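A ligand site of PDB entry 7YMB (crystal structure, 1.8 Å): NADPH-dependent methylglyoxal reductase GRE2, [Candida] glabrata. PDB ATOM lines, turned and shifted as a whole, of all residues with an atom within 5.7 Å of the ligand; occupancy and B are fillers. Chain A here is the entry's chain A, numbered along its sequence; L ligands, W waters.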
ATOM      1  N   GLY A  14       6.753 -15.645  19.501  1.00  0.00           N
ATOM      2  CA  GLY A  14       5.360 -15.377  19.179  1.00  0.00           C
ATOM      3  C   GLY A  14       5.102 -13.923  18.858  1.00  0.00           C
ATOM      4  O   GLY A  14       4.138 -13.330  19.362  1.00  0.00           O
ATOM      5  N   ALA A  15       5.951 -13.350  18.001  1.00  0.00           N
ATOM      6  CA  ALA A  15       5.965 -11.915  17.773  1.00  0.00           C
ATOM      7  C   ALA A  15       4.692 -11.391  17.123  1.00  0.00           C
ATOM      8  O   ALA A  15       4.426 -10.191  17.195  1.00  0.00           O
ATOM      9  CB  ALA A  15       7.173 -11.539  16.907  1.00  0.00           C
ATOM     10  N   SER A  16       3.913 -12.254  16.478  1.00  0.00           N
ATOM     11  CA  SER A  16       2.724 -11.750  15.804  1.00  0.00           C
ATOM     12  C   SER A  16       1.543 -11.547  16.735  1.00  0.00           C
ATOM     13  O   SER A  16       0.537 -10.985  16.311  1.00  0.00           O
ATOM     14  CB  SER A  16       2.333 -12.703  14.671  1.00  0.00           C
ATOM     15  OG  SER A  16       2.280 -14.040  15.125  1.00  0.00           O
ATOM     16  N   GLY A  17       1.634 -12.006  18.012  1.00  0.00           N
ATOM     17  CA  GLY A  17       0.470 -11.997  18.881  1.00  0.00           C
ATOM     18  C   GLY A  17       0.140 -10.613  19.480  1.00  0.00           C
ATOM     19  O   GLY A  17       0.886  -9.649  19.369  1.00  0.00           O
ATOM     20  N   PHE A  18      -1.025 -10.571  20.121  1.00  0.00           N
ATOM     21  CA  PHE A  18      -1.582  -9.337  20.684  1.00  0.00           C
ATOM     22  C   PHE A  18      -0.635  -8.689  21.680  1.00  0.00           C
ATOM     23  O   PHE A  18      -0.273  -7.512  21.554  1.00  0.00           O
ATOM     24  CB  PHE A  18      -2.923  -9.680  21.338  1.00  0.00           C
ATOM     25  CG  PHE A  18      -3.571  -8.572  22.159  1.00  0.00           C
ATOM     26  CD1 PHE A  18      -3.916  -7.355  21.587  1.00  0.00           C
ATOM     27  CD2 PHE A  18      -3.919  -8.821  23.480  1.00  0.00           C
ATOM     28  CE1 PHE A  18      -4.556  -6.374  22.347  1.00  0.00           C
ATOM     29  CE2 PHE A  18      -4.553  -7.848  24.241  1.00  0.00           C
ATOM     30  CZ  PHE A  18      -4.874  -6.613  23.678  1.00  0.00           C
ATOM     31  N   ILE A  19      -0.245  -9.441  22.709  1.00  0.00           N
ATOM     32  CA  ILE A  19       0.633  -8.886  23.728  1.00  0.00           C
ATOM     33  C   ILE A  19       2.035  -8.643  23.162  1.00  0.00           C
ATOM     34  O   ILE A  19       2.647  -7.588  23.397  1.00  0.00           O
ATOM     35  CB  ILE A  19       0.671  -9.831  24.945  1.00  0.00           C
ATOM     36  CG1 ILE A  19      -0.682  -9.769  25.669  1.00  0.00           C
ATOM     37  CG2 ILE A  19       1.800  -9.461  25.889  1.00  0.00           C
ATOM     38  CD1 ILE A  19      -0.821 -10.800  26.802  1.00  0.00           C
ATOM     39  N   ALA A  20       2.553  -9.587  22.392  1.00  0.00           N
ATOM     40  CA  ALA A  20       3.925  -9.473  21.906  1.00  0.00           C
ATOM     41  C   ALA A  20       4.106  -8.268  20.970  1.00  0.00           C
ATOM     42  O   ALA A  20       5.164  -7.633  20.981  1.00  0.00           O
ATOM     43  CB  ALA A  20       4.335 -10.771  21.206  1.00  0.00           C
ATOM     44  N   ARG A  39       5.248 -18.061  12.883  1.00  0.00           N
ATOM     45  CA  ARG A  39       5.014 -19.388  12.348  1.00  0.00           C
ATOM     46  C   ARG A  39       5.035 -19.447  10.820  1.00  0.00           C
ATOM     47  O   ARG A  39       4.981 -20.558  10.268  1.00  0.00           O
ATOM     48  CB  ARG A  39       3.675 -19.963  12.865  1.00  0.00           C
ATOM     49  CG  ARG A  39       3.530 -19.954  14.387  1.00  0.00           C
ATOM     50  CD  ARG A  39       2.162 -20.478  14.815  1.00  0.00           C
ATOM     51  NE  ARG A  39       2.179 -21.924  14.863  1.00  0.00           N
ATOM     52  CZ  ARG A  39       1.250 -22.674  15.441  1.00  0.00           C
ATOM     53  NH1 ARG A  39       0.189 -22.109  16.017  1.00  0.00           N
ATOM     54  NH2 ARG A  39       1.374 -23.998  15.424  1.00  0.00           N
ATOM     55  N   LYS A  43       3.144 -14.122   7.971  1.00  0.00           N
ATOM     56  CA  LYS A  43       3.089 -13.356   9.209  1.00  0.00           C
ATOM     57  C   LYS A  43       4.349 -12.534   9.431  1.00  0.00           C
ATOM     58  O   LYS A  43       4.281 -11.364   9.818  1.00  0.00           O
ATOM     59  CB  LYS A  43       2.856 -14.293  10.406  1.00  0.00           C
ATOM     60  CG  LYS A  43       1.395 -14.702  10.600  1.00  0.00           C
ATOM     61  CD  LYS A  43       1.291 -16.084  11.273  1.00  0.00           C
ATOM     62  CE  LYS A  43      -0.147 -16.614  11.314  1.00  0.00           C
ATOM     63  NZ  LYS A  43      -0.203 -17.979  11.965  1.00  0.00           N
ATOM     64  N   VAL A  62       9.672 -20.031  13.629  1.00  0.00           N
ATOM     65  CA  VAL A  62       9.586 -21.162  14.546  1.00  0.00           C
ATOM     66  C   VAL A  62       8.159 -21.656  14.400  1.00  0.00           C
ATOM     67  O   VAL A  62       7.223 -21.046  14.954  1.00  0.00           O
ATOM     68  CB  VAL A  62       9.909 -20.797  16.000  1.00  0.00           C
ATOM     69  CG1 VAL A  62       9.768 -22.027  16.921  1.00  0.00           C
ATOM     70  CG2 VAL A  62      11.314 -20.203  16.110  1.00  0.00           C
ATOM     71  N   LYS A  63       7.968 -22.727  13.636  1.00  0.00           N
ATOM     72  CA  LYS A  63       6.637 -23.125  13.175  1.00  0.00           C
ATOM     73  C   LYS A  63       5.788 -23.687  14.304  1.00  0.00           C
ATOM     74  O   LYS A  63       4.563 -23.495  14.293  1.00  0.00           O
ATOM     75  CB  LYS A  63       6.751 -24.149  12.049  1.00  0.00           C
ATOM     76  CG  LYS A  63       7.029 -23.566  10.674  1.00  0.00           C
ATOM     77  CD  LYS A  63       7.486 -24.638   9.689  1.00  0.00           C
ATOM     78  CE  LYS A  63       6.877 -24.387   8.325  1.00  0.00           C
ATOM     79  NZ  LYS A  63       7.728 -24.908   7.209  1.00  0.00           N
ATOM     80  N   ASP A  64       6.400 -24.400  15.253  1.00  0.00           N
ATOM     81  CA  ASP A  64       5.639 -25.046  16.327  1.00  0.00           C
ATOM     82  C   ASP A  64       6.528 -25.191  17.554  1.00  0.00           C
ATOM     83  O   ASP A  64       7.537 -25.894  17.513  1.00  0.00           O
ATOM     84  CB  ASP A  64       5.116 -26.418  15.890  1.00  0.00           C
ATOM     85  CG  ASP A  64       4.163 -27.033  16.912  1.00  0.00           C
ATOM     86  OD1 ASP A  64       3.983 -26.475  18.005  1.00  0.00           O
ATOM     87  OD2 ASP A  64       3.576 -28.098  16.599  1.00  0.00           O
ATOM     88  N   ILE A  65       6.143 -24.505  18.641  1.00  0.00           N
ATOM     89  CA  ILE A  65       6.935 -24.558  19.870  1.00  0.00           C
ATOM     90  C   ILE A  65       6.812 -25.868  20.611  1.00  0.00           C
ATOM     91  O   ILE A  65       7.593 -26.114  21.546  1.00  0.00           O
ATOM     92  CB  ILE A  65       6.548 -23.397  20.814  1.00  0.00           C
ATOM     93  CG1 ILE A  65       5.079 -23.517  21.227  1.00  0.00           C
ATOM     94  CG2 ILE A  65       6.838 -22.056  20.164  1.00  0.00           C
ATOM     95  CD1 ILE A  65       4.599 -22.365  22.128  1.00  0.00           C
ATOM     96  N   ALA A  66       5.856 -26.726  20.254  1.00  0.00           N
ATOM     97  CA  ALA A  66       5.763 -28.018  20.912  1.00  0.00           C
ATOM     98  C   ALA A  66       6.847 -28.984  20.469  1.00  0.00           C
ATOM     99  O   ALA A  66       7.002 -30.057  21.063  1.00  0.00           O
ATOM    100  CB  ALA A  66       4.385 -28.631  20.665  1.00  0.00           C
ATOM    101  N   THR A  88       6.914 -15.323  25.104  1.00  0.00           N
ATOM    102  CA  THR A  88       5.499 -15.010  25.261  1.00  0.00           C
ATOM    103  C   THR A  88       4.580 -16.012  24.572  1.00  0.00           C
ATOM    104  O   THR A  88       3.380 -16.008  24.854  1.00  0.00           O
ATOM    105  CB  THR A  88       5.160 -13.599  24.731  1.00  0.00           C
ATOM    106  OG1 THR A  88       5.019 -13.640  23.306  1.00  0.00           O
ATOM    107  CG2 THR A  88       6.250 -12.561  25.107  1.00  0.00           C
ATOM    108  N   ALA A  89       5.115 -16.865  23.698  1.00  0.00           N
ATOM    109  CA  ALA A  89       4.279 -17.686  22.813  1.00  0.00           C
ATOM    110  C   ALA A  89       3.700 -18.892  23.543  1.00  0.00           C
ATOM    111  O   ALA A  89       4.452 -19.733  24.051  1.00  0.00           O
ATOM    112  CB  ALA A  89       5.097 -18.148  21.605  1.00  0.00           C
ATOM    113  N   SER A  90       2.356 -19.029  23.507  1.00  0.00           N
ATOM    114  CA  SER A  90       1.713 -20.210  24.069  1.00  0.00           C
ATOM    115  C   SER A  90       0.285 -20.232  23.558  1.00  0.00           C
ATOM    116  O   SER A  90      -0.308 -19.163  23.385  1.00  0.00           O
ATOM    117  CB  SER A  90       1.739 -20.166  25.612  1.00  0.00           C
ATOM    118  OG  SER A  90       1.426 -21.424  26.198  1.00  0.00           O
ATOM    119  N   PRO A  91      -0.297 -21.410  23.272  1.00  0.00           N
ATOM    120  CA  PRO A  91      -1.643 -21.437  22.693  1.00  0.00           C
ATOM    121  C   PRO A  91      -2.703 -20.960  23.667  1.00  0.00           C
ATOM    122  O   PRO A  91      -2.803 -21.452  24.801  1.00  0.00           O
ATOM    123  CB  PRO A  91      -1.836 -22.915  22.324  1.00  0.00           C
ATOM    124  CG  PRO A  91      -0.915 -23.644  23.236  1.00  0.00           C
ATOM    125  CD  PRO A  91       0.271 -22.768  23.427  1.00  0.00           C
ATOM    126  N   LEU A  92      -3.491 -19.984  23.229  1.00  0.00           N
ATOM    127  CA  LEU A  92      -4.665 -19.472  23.940  1.00  0.00           C
ATOM    128  C   LEU A  92      -5.880 -19.602  23.028  1.00  0.00           C
ATOM    129  O   LEU A  92      -6.150 -18.720  22.206  1.00  0.00           O
ATOM    130  CB  LEU A  92      -4.438 -18.018  24.385  1.00  0.00           C
ATOM    131  CG  LEU A  92      -5.627 -17.273  25.020  1.00  0.00           C
ATOM    132  CD1 LEU A  92      -6.208 -17.900  26.270  1.00  0.00           C
ATOM    133  CD2 LEU A  92      -5.189 -15.862  25.306  1.00  0.00           C
ATOM    134  N   PRO A 106       2.159 -28.078  24.218  1.00  0.00           N
ATOM    135  CA  PRO A 106       2.882 -26.949  23.606  1.00  0.00           C
ATOM    136  C   PRO A 106       3.265 -25.855  24.597  1.00  0.00           C
ATOM    137  O   PRO A 106       4.353 -25.294  24.488  1.00  0.00           O
ATOM    138  CB  PRO A 106       1.887 -26.432  22.542  1.00  0.00           C
ATOM    139  CG  PRO A 106       0.929 -27.564  22.306  1.00  0.00           C
ATOM    140  CD  PRO A 106       0.809 -28.243  23.630  1.00  0.00           C
ATOM    141  N   THR A 132       6.002 -14.957  29.886  1.00  0.00           N
ATOM    142  CA  THR A 132       4.604 -14.525  30.035  1.00  0.00           C
ATOM    143  C   THR A 132       3.818 -15.687  30.630  1.00  0.00           C
ATOM    144  O   THR A 132       3.538 -16.671  29.940  1.00  0.00           O
ATOM    145  CB  THR A 132       3.985 -14.129  28.698  1.00  0.00           C
ATOM    146  OG1 THR A 132       4.856 -13.229  28.015  1.00  0.00           O
ATOM    147  CG2 THR A 132       2.638 -13.440  28.932  1.00  0.00           C
ATOM    148  N   SER A 133       3.464 -15.569  31.905  1.00  0.00           N
ATOM    149  CA  SER A 133       2.633 -16.568  32.565  1.00  0.00           C
ATOM    150  C   SER A 133       1.191 -16.065  32.591  1.00  0.00           C
ATOM    151  O   SER A 133       0.729 -15.489  31.607  1.00  0.00           O
ATOM    152  CB  SER A 133       3.191 -16.846  33.973  1.00  0.00           C
ATOM    153  OG  SER A 133       2.401 -17.752  34.721  1.00  0.00           O
ATOM    154  N   SER A 134       0.459 -16.246  33.696  1.00  0.00           N
ATOM    155  CA  SER A 134      -0.916 -15.768  33.738  1.00  0.00           C
ATOM    156  C   SER A 134      -1.417 -15.758  35.177  1.00  0.00           C
ATOM    157  O   SER A 134      -0.907 -16.472  36.032  1.00  0.00           O
ATOM    158  CB  SER A 134      -1.847 -16.660  32.890  1.00  0.00           C
ATOM    159  OG  SER A 134      -3.225 -16.360  33.111  1.00  0.00           O
ATOM    160  N   PHE A 135      -2.451 -14.944  35.402  1.00  0.00           N
ATOM    161  CA  PHE A 135      -3.297 -15.127  36.585  1.00  0.00           C
ATOM    162  C   PHE A 135      -3.721 -16.587  36.732  1.00  0.00           C
ATOM    163  O   PHE A 135      -3.880 -17.084  37.854  1.00  0.00           O
ATOM    164  CB  PHE A 135      -4.493 -14.180  36.450  1.00  0.00           C
ATOM    165  CG  PHE A 135      -5.548 -14.334  37.500  1.00  0.00           C
ATOM    166  CD1 PHE A 135      -5.366 -13.828  38.776  1.00  0.00           C
ATOM    167  CD2 PHE A 135      -6.743 -14.954  37.199  1.00  0.00           C
ATOM    168  CE1 PHE A 135      -6.352 -13.951  39.732  1.00  0.00           C
ATOM    169  CE2 PHE A 135      -7.737 -15.081  38.166  1.00  0.00           C
ATOM    170  CZ  PHE A 135      -7.528 -14.582  39.433  1.00  0.00           C
ATOM    171  N   TYR A 172      -6.539 -24.870  29.534  1.00  0.00           N
ATOM    172  CA  TYR A 172      -5.632 -23.769  29.236  1.00  0.00           C
ATOM    173  C   TYR A 172      -5.057 -23.165  30.520  1.00  0.00           C
ATOM    174  O   TYR A 172      -3.869 -22.846  30.594  1.00  0.00           O
ATOM    175  CB  TYR A 172      -6.348 -22.688  28.420  1.00  0.00           C
ATOM    176  CG  TYR A 172      -5.610 -21.369  28.487  1.00  0.00           C
ATOM    177  CD1 TYR A 172      -4.473 -21.147  27.713  1.00  0.00           C
ATOM    178  CD2 TYR A 172      -6.016 -20.367  29.363  1.00  0.00           C
ATOM    179  CE1 TYR A 172      -3.782 -19.958  27.779  1.00  0.00           C
ATOM    180  CE2 TYR A 172      -5.311 -19.177  29.450  1.00  0.00           C
ATOM    181  CZ  TYR A 172      -4.193 -18.985  28.649  1.00  0.00           C
ATOM    182  OH  TYR A 172      -3.525 -17.792  28.754  1.00  0.00           O
ATOM    183  N   LYS A 176      -0.851 -22.885  31.564  1.00  0.00           N
ATOM    184  CA  LYS A 176      -0.043 -21.771  32.070  1.00  0.00           C
ATOM    185  C   LYS A 176       0.668 -22.148  33.366  1.00  0.00           C
ATOM    186  O   LYS A 176       1.856 -21.834  33.551  1.00  0.00           O
ATOM    187  CB  LYS A 176      -0.950 -20.553  32.289  1.00  0.00           C
ATOM    188  CG  LYS A 176      -1.668 -20.132  30.995  1.00  0.00           C
ATOM    189  CD  LYS A 176      -0.693 -19.834  29.820  1.00  0.00           C
ATOM    190  CE  LYS A 176       0.296 -18.704  30.137  1.00  0.00           C
ATOM    191  NZ  LYS A 176       1.332 -18.505  29.070  1.00  0.00           N
ATOM    192  N   ASP A 202       2.420 -11.993  34.888  1.00  0.00           N
ATOM    193  CA  ASP A 202       1.308 -12.921  35.092  1.00  0.00           C
ATOM    194  C   ASP A 202       0.004 -12.115  34.986  1.00  0.00           C
ATOM    195  O   ASP A 202      -0.497 -11.642  36.000  1.00  0.00           O
ATOM    196  CB  ASP A 202       1.338 -13.585  36.480  1.00  0.00           C
ATOM    197  CG  ASP A 202       2.711 -14.160  36.867  1.00  0.00           C
ATOM    198  OD1 ASP A 202       3.604 -14.301  36.019  1.00  0.00           O
ATOM    199  OD2 ASP A 202       2.840 -14.649  38.039  1.00  0.00           O
ATOM    200  N   PRO A 203      -0.551 -11.946  33.777  1.00  0.00           N
ATOM    201  CA  PRO A 203      -1.704 -11.047  33.621  1.00  0.00           C
ATOM    202  C   PRO A 203      -3.040 -11.726  33.880  1.00  0.00           C
ATOM    203  O   PRO A 203      -3.208 -12.937  33.684  1.00  0.00           O
ATOM    204  CB  PRO A 203      -1.630 -10.622  32.132  1.00  0.00           C
ATOM    205  CG  PRO A 203      -0.202 -10.966  31.677  1.00  0.00           C
ATOM    206  CD  PRO A 203       0.113 -12.223  32.486  1.00  0.00           C
ATOM    207  N   VAL A 204      -4.011 -10.898  34.278  1.00  0.00           N
ATOM    208  CA  VAL A 204      -5.414 -11.271  34.246  1.00  0.00           C
ATOM    209  C   VAL A 204      -5.866 -11.137  32.793  1.00  0.00           C
ATOM    210  O   VAL A 204      -5.031 -11.180  31.887  1.00  0.00           O
ATOM    211  CB  VAL A 204      -6.249 -10.411  35.210  1.00  0.00           C
ATOM    212  CG1 VAL A 204      -5.904 -10.798  36.677  1.00  0.00           C
ATOM    213  CG2 VAL A 204      -5.977  -8.911  34.981  1.00  0.00           C
ATOM    214  N   TYR A 205      -7.177 -11.020  32.548  1.00  0.00           N
ATOM    215  CA  TYR A 205      -7.635 -10.779  31.170  1.00  0.00           C
ATOM    216  C   TYR A 205      -7.056  -9.463  30.645  1.00  0.00           C
ATOM    217  O   TYR A 205      -7.160  -8.429  31.304  1.00  0.00           O
ATOM    218  CB  TYR A 205      -9.151 -10.698  31.095  1.00  0.00           C
ATOM    219  CG  TYR A 205      -9.866 -12.019  30.998  1.00  0.00           C
ATOM    220  CD1 TYR A 205      -9.597 -13.035  31.891  1.00  0.00           C
ATOM    221  CD2 TYR A 205     -10.813 -12.250  30.009  1.00  0.00           C
ATOM    222  CE1 TYR A 205     -10.282 -14.270  31.822  1.00  0.00           C
ATOM    223  CE2 TYR A 205     -11.501 -13.464  29.927  1.00  0.00           C
ATOM    224  CZ  TYR A 205     -11.230 -14.464  30.837  1.00  0.00           C
ATOM    225  OH  TYR A 205     -11.901 -15.669  30.744  1.00  0.00           O
ATOM    226  N   VAL A 206      -6.496  -9.501  29.446  1.00  0.00           N
ATOM    227  CA  VAL A 206      -5.776  -8.363  28.893  1.00  0.00           C
ATOM    228  C   VAL A 206      -6.658  -7.707  27.832  1.00  0.00           C
ATOM    229  O   VAL A 206      -6.994  -8.335  26.812  1.00  0.00           O
ATOM    230  CB  VAL A 206      -4.411  -8.770  28.323  1.00  0.00           C
ATOM    231  CG1 VAL A 206      -3.688  -7.544  27.777  1.00  0.00           C
ATOM    232  CG2 VAL A 206      -3.552  -9.421  29.434  1.00  0.00           C
ATOM    233  N   ASN A 221      -7.937 -11.905  18.882  1.00  0.00           N
ATOM    234  CA  ASN A 221      -7.473 -12.839  19.910  1.00  0.00           C
ATOM    235  C   ASN A 221      -8.523 -12.996  20.991  1.00  0.00           C
ATOM    236  O   ASN A 221      -9.404 -12.147  21.166  1.00  0.00           O
ATOM    237  CB  ASN A 221      -6.168 -12.331  20.536  1.00  0.00           C
ATOM    238  CG  ASN A 221      -6.298 -10.912  21.054  1.00  0.00           C
ATOM    239  OD1 ASN A 221      -6.393  -9.965  20.270  1.00  0.00           O
ATOM    240  ND2 ASN A 221      -6.324 -10.760  22.366  1.00  0.00           N
ATOM    241  N   VAL A 222      -8.384 -14.083  21.778  1.00  0.00           N
ATOM    242  CA  VAL A 222      -9.444 -14.494  22.705  1.00  0.00           C
ATOM    243  C   VAL A 222      -9.836 -13.360  23.653  1.00  0.00           C
ATOM    244  O   VAL A 222     -11.022 -13.031  23.785  1.00  0.00           O
ATOM    245  CB  VAL A 222      -9.025 -15.746  23.487  1.00  0.00           C
ATOM    246  CG1 VAL A 222      -9.984 -15.961  24.650  1.00  0.00           C
ATOM    247  CG2 VAL A 222      -9.055 -16.966  22.568  1.00  0.00           C
ATOM    248  N   SER A 223      -8.876 -12.778  24.367  1.00  0.00           N
ATOM    249  CA  SER A 223      -9.280 -11.801  25.378  1.00  0.00           C
ATOM    250  C   SER A 223      -9.906 -10.569  24.724  1.00  0.00           C
ATOM    251  O   SER A 223     -10.943 -10.068  25.189  1.00  0.00           O
ATOM    252  CB  SER A 223      -8.077 -11.405  26.250  1.00  0.00           C
ATOM    253  OG  SER A 223      -7.097 -10.713  25.490  1.00  0.00           O
HETATM  254  P1  LIG L   1      -2.405 -14.307  20.885  1.00  0.00           P
HETATM  255  O1  LIG L   1      -2.593 -12.972  20.240  1.00  0.00           O
HETATM  256  O2  LIG L   1      -3.249 -15.455  20.393  1.00  0.00           O
HETATM  257  O3  LIG L   1      -0.836 -14.608  20.822  1.00  0.00           O
HETATM  258  C1  LIG L   1      -0.677 -15.998  20.847  1.00  0.00           C
HETATM  259  C2  LIG L   1       0.679 -16.219  20.188  1.00  0.00           C
HETATM  260  O4  LIG L   1       1.152 -17.516  20.432  1.00  0.00           O
HETATM  261  C3  LIG L   1       0.461 -16.008  18.681  1.00  0.00           C
HETATM  262  O5  LIG L   1       1.550 -15.275  18.152  1.00  0.00           O
HETATM  263  C4  LIG L   1       0.497 -17.468  18.156  1.00  0.00           C
HETATM  264  O6  LIG L   1       1.025 -17.604  16.940  1.00  0.00           O
HETATM  265  C5  LIG L   1       1.524 -18.055  19.191  1.00  0.00           C
HETATM  266  N1  LIG L   1       1.440 -19.524  19.290  1.00  0.00           N
HETATM  267  C6  LIG L   1       0.418 -20.296  19.889  1.00  0.00           C
HETATM  268  N2  LIG L   1       0.667 -21.634  19.797  1.00  0.00           N
HETATM  269  C7  LIG L   1       1.886 -21.706  19.121  1.00  0.00           C
HETATM  270  C8  LIG L   1       2.668 -22.809  18.719  1.00  0.00           C
HETATM  271  N3  LIG L   1       2.254 -24.091  19.000  1.00  0.00           N
HETATM  272  N4  LIG L   1       3.846 -22.637  18.065  1.00  0.00           N
HETATM  273  C9  LIG L   1       4.202 -21.336  17.829  1.00  0.00           C
HETATM  274  N5  LIG L   1       3.565 -20.188  18.138  1.00  0.00           N
HETATM  275  C10 LIG L   1       2.392 -20.403  18.809  1.00  0.00           C
HETATM  276  O7  LIG L   1      -2.994 -14.153  22.440  1.00  0.00           O
HETATM  277  P2  LIG L   1      -2.151 -13.266  23.539  1.00  0.00           P
HETATM  278  O8  LIG L   1      -1.213 -12.274  22.985  1.00  0.00           O
HETATM  279  O9  LIG L   1      -3.166 -12.867  24.587  1.00  0.00           O
HETATM  280  O10 LIG L   1      -1.236 -14.424  24.394  1.00  0.00           O
HETATM  281  C11 LIG L   1       0.113 -14.156  24.389  1.00  0.00           C
HETATM  282  C12 LIG L   1       0.695 -14.748  25.724  1.00  0.00           C
HETATM  283  O11 LIG L   1       0.048 -14.065  26.833  1.00  0.00           O
HETATM  284  C13 LIG L   1       0.338 -16.251  25.920  1.00  0.00           C
HETATM  285  O12 LIG L   1       1.398 -16.883  26.640  1.00  0.00           O
HETATM  286  C14 LIG L   1      -0.891 -16.194  26.831  1.00  0.00           C
HETATM  287  O13 LIG L   1      -1.026 -17.319  27.624  1.00  0.00           O
HETATM  288  C15 LIG L   1      -0.466 -15.026  27.730  1.00  0.00           C
HETATM  289  N6  LIG L   1      -1.638 -14.391  28.434  1.00  0.00           N
HETATM  290  C16 LIG L   1      -2.655 -13.711  27.759  1.00  0.00           C
HETATM  291  C17 LIG L   1      -3.688 -13.174  28.482  1.00  0.00           C
HETATM  292  C18 LIG L   1      -4.793 -12.449  27.837  1.00  0.00           C
HETATM  293  O14 LIG L   1      -5.820 -12.147  28.455  1.00  0.00           O
HETATM  294  N7  LIG L   1      -4.700 -12.075  26.478  1.00  0.00           N
HETATM  295  C19 LIG L   1      -3.783 -13.296  29.964  1.00  0.00           C
HETATM  296  C20 LIG L   1      -2.608 -13.932  30.567  1.00  0.00           C
HETATM  297  C21 LIG L   1      -1.634 -14.435  29.847  1.00  0.00           C
HETATM  298  P3  LIG L   1      -0.067 -17.208  15.556  1.00  0.00           P
HETATM  299  O15 LIG L   1      -1.309 -17.877  16.061  1.00  0.00           O
HETATM  300  O16 LIG L   1       0.632 -17.836  14.350  1.00  0.00           O
HETATM  301  O17 LIG L   1       0.018 -15.700  15.674  1.00  0.00           O
HETATM  302  O   HOH W   1       3.289 -16.447  14.281  1.00  0.00           O
HETATM  303  O   HOH W   2       2.929 -14.271  21.599  1.00  0.00           O
HETATM  304  O   HOH W   3      -3.766 -17.046  18.410  1.00  0.00           O
HETATM  305  O   HOH W   4      -3.371 -12.559  17.600  1.00  0.00           O
HETATM  306  O   HOH W   5       0.978 -27.236  18.412  1.00  0.00           O
HETATM  307  O   HOH W   6       1.301 -12.113  22.035  1.00  0.00           O
HETATM  308  O   HOH W   7       4.631 -17.874  17.034  1.00  0.00           O
HETATM  309  O   HOH W   8      -5.844 -15.693  21.706  1.00  0.00           O
HETATM  310  O   HOH W   9      -8.063 -14.555  28.500  1.00  0.00           O
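CD of Arg 39 touches O16 of the ligand (3.1 Å). Lys 63 touches the ligand (O to N4, 3.9 Å). CA of Ala 89 touches O4 of the ligand, at 3.9 Å. Ser 90 touches the ligand (CB to O12, 3.5 Å). N of Pro 91 touches N2 of the ligand (3.6 Å). CD2 of Leu 92 touches O9 of the ligand, 3.7 Å away. CG2 of Thr 132 touches O11 of the ligand (3.4 Å). Ser 133 touches the ligand (O to C21, 3.1 Å). Ser 134 touches the ligand (OG to C20, 3.6 Å). Pro 203 touches the ligand (O to C20, 3.3 Å). Val 204 touches the ligand. CA of Tyr 205 touches O14 of the ligand, 3.5 Å away. CB of Asn 221 touches O1 of the ligand (3.6 Å). Hydrophobic or aromatic side chains within 4 Å of the ligand: Phe 18, Ile 19, Ile 65, Pro 91, Leu 92, Tyr 172, Pro 203 and Val 206. Within 4 Å of the ligand: Gly 14, Ser 16, Gly 17, Phe 18, Ile 19, Arg 39, Lys 43, Lys 63, Asp 64, Ile 65, Thr 88, Ala 89, Ser 90, Pro 91, Leu 92, Thr 132, Ser 133, Ser 134, Tyr 172, Lys 176, Pro 203, Val 204, Tyr 205, Val 206, Asn 221 and Ser 223. The nearest printed residue that does not touch the ligand is Val 62 (4.2 Å).
Water W8 lies within hydrogen-bond range of an oxygen (O2) of the ligand (2.9 Å), the backbone NH of Val 222 (3.0 Å) and the backbone carbonyl oxygen of Leu 92 (3.1 Å). Water W1 lies within hydrogen-bond range of OG of Ser 16 (2.7 Å), N of Arg 39 (2.9 Å) and O16 of the ligand (3.0 Å). Water W2 lies within hydrogen-bond range of the backbone carbonyl oxygen of Gly 14 and the side-chain hydroxyl of Thr 88. Water W5 lies within hydrogen-bond range of OD1 of Asp 64 and N3 of the ligand.
NZ of Lys 43 is in salt-bridge range of O16 of the ligand (2.5 Å). OH of Tyr 172 lies within hydrogen-bond range of O13 of the ligand (2.8 Å). The backbone carbonyl oxygen (O) of Thr 88 sits at hydrogen-bond distance from an oxygen (O12) of the ligand (2.8 Å). An oxygen (O17) of the ligand lies within hydrogen-bond range of the side-chain hydroxyl (OG) of Ser 16 (2.9 Å). N of Phe 18 sits at hydrogen-bond distance from O1 of the ligand. An oxygen (O14) of the ligand lies within hydrogen-bond range of the backbone NH (N) of Val 206. O12 of the ligand sits at hydrogen-bond distance from NZ of Lys 176 (2.9 Å). OG of Ser 223 sits at hydrogen-bond distance from N7 of the ligand, 2.9 Å away. O8 of the ligand lies within hydrogen-bond range of N of Ile 19 (3.0 Å). N of Ile 65 lies within hydrogen-bond range of N4 of the ligand. N3 of the ligand lies within hydrogen-bond range of OD1 of Asp 64 (3.1 Å). The backbone NH (N) of Gly 17 lies within hydrogen-bond range of an oxygen (O5) of the ligand (3.3 Å). O of Gly 14 lies within hydrogen-bond range of O5 of the ligand (3.5 Å).
The side-chain hydroxyl (OG) of Ser 223 sits at hydrogen-bond distance from the backbone carbonyl oxygen (O) of Val 206, 2.7 Å away. O of Thr 132 lies within hydrogen-bond range of NZ of Lys 176 (3.0 Å). OG of Ser 223 lies within hydrogen-bond range of ND2 of Asn 221, 3.2 Å away. The guanidinium group (NE) of Arg 39 lies within hydrogen-bond range of the backbone carbonyl oxygen (O) of Lys 63. The side-chain carboxylate (OD1) of Asp 64 sits at hydrogen-bond distance from the backbone NH (N) of Ala 66, 2.9 Å away. OG of Ser 134 lies within hydrogen-bond range of O of Pro 203. The backbone carbonyl oxygen (O) of Pro 203 sits at hydrogen-bond distance from the backbone NH (N) of Phe 135, at 2.7 Å.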
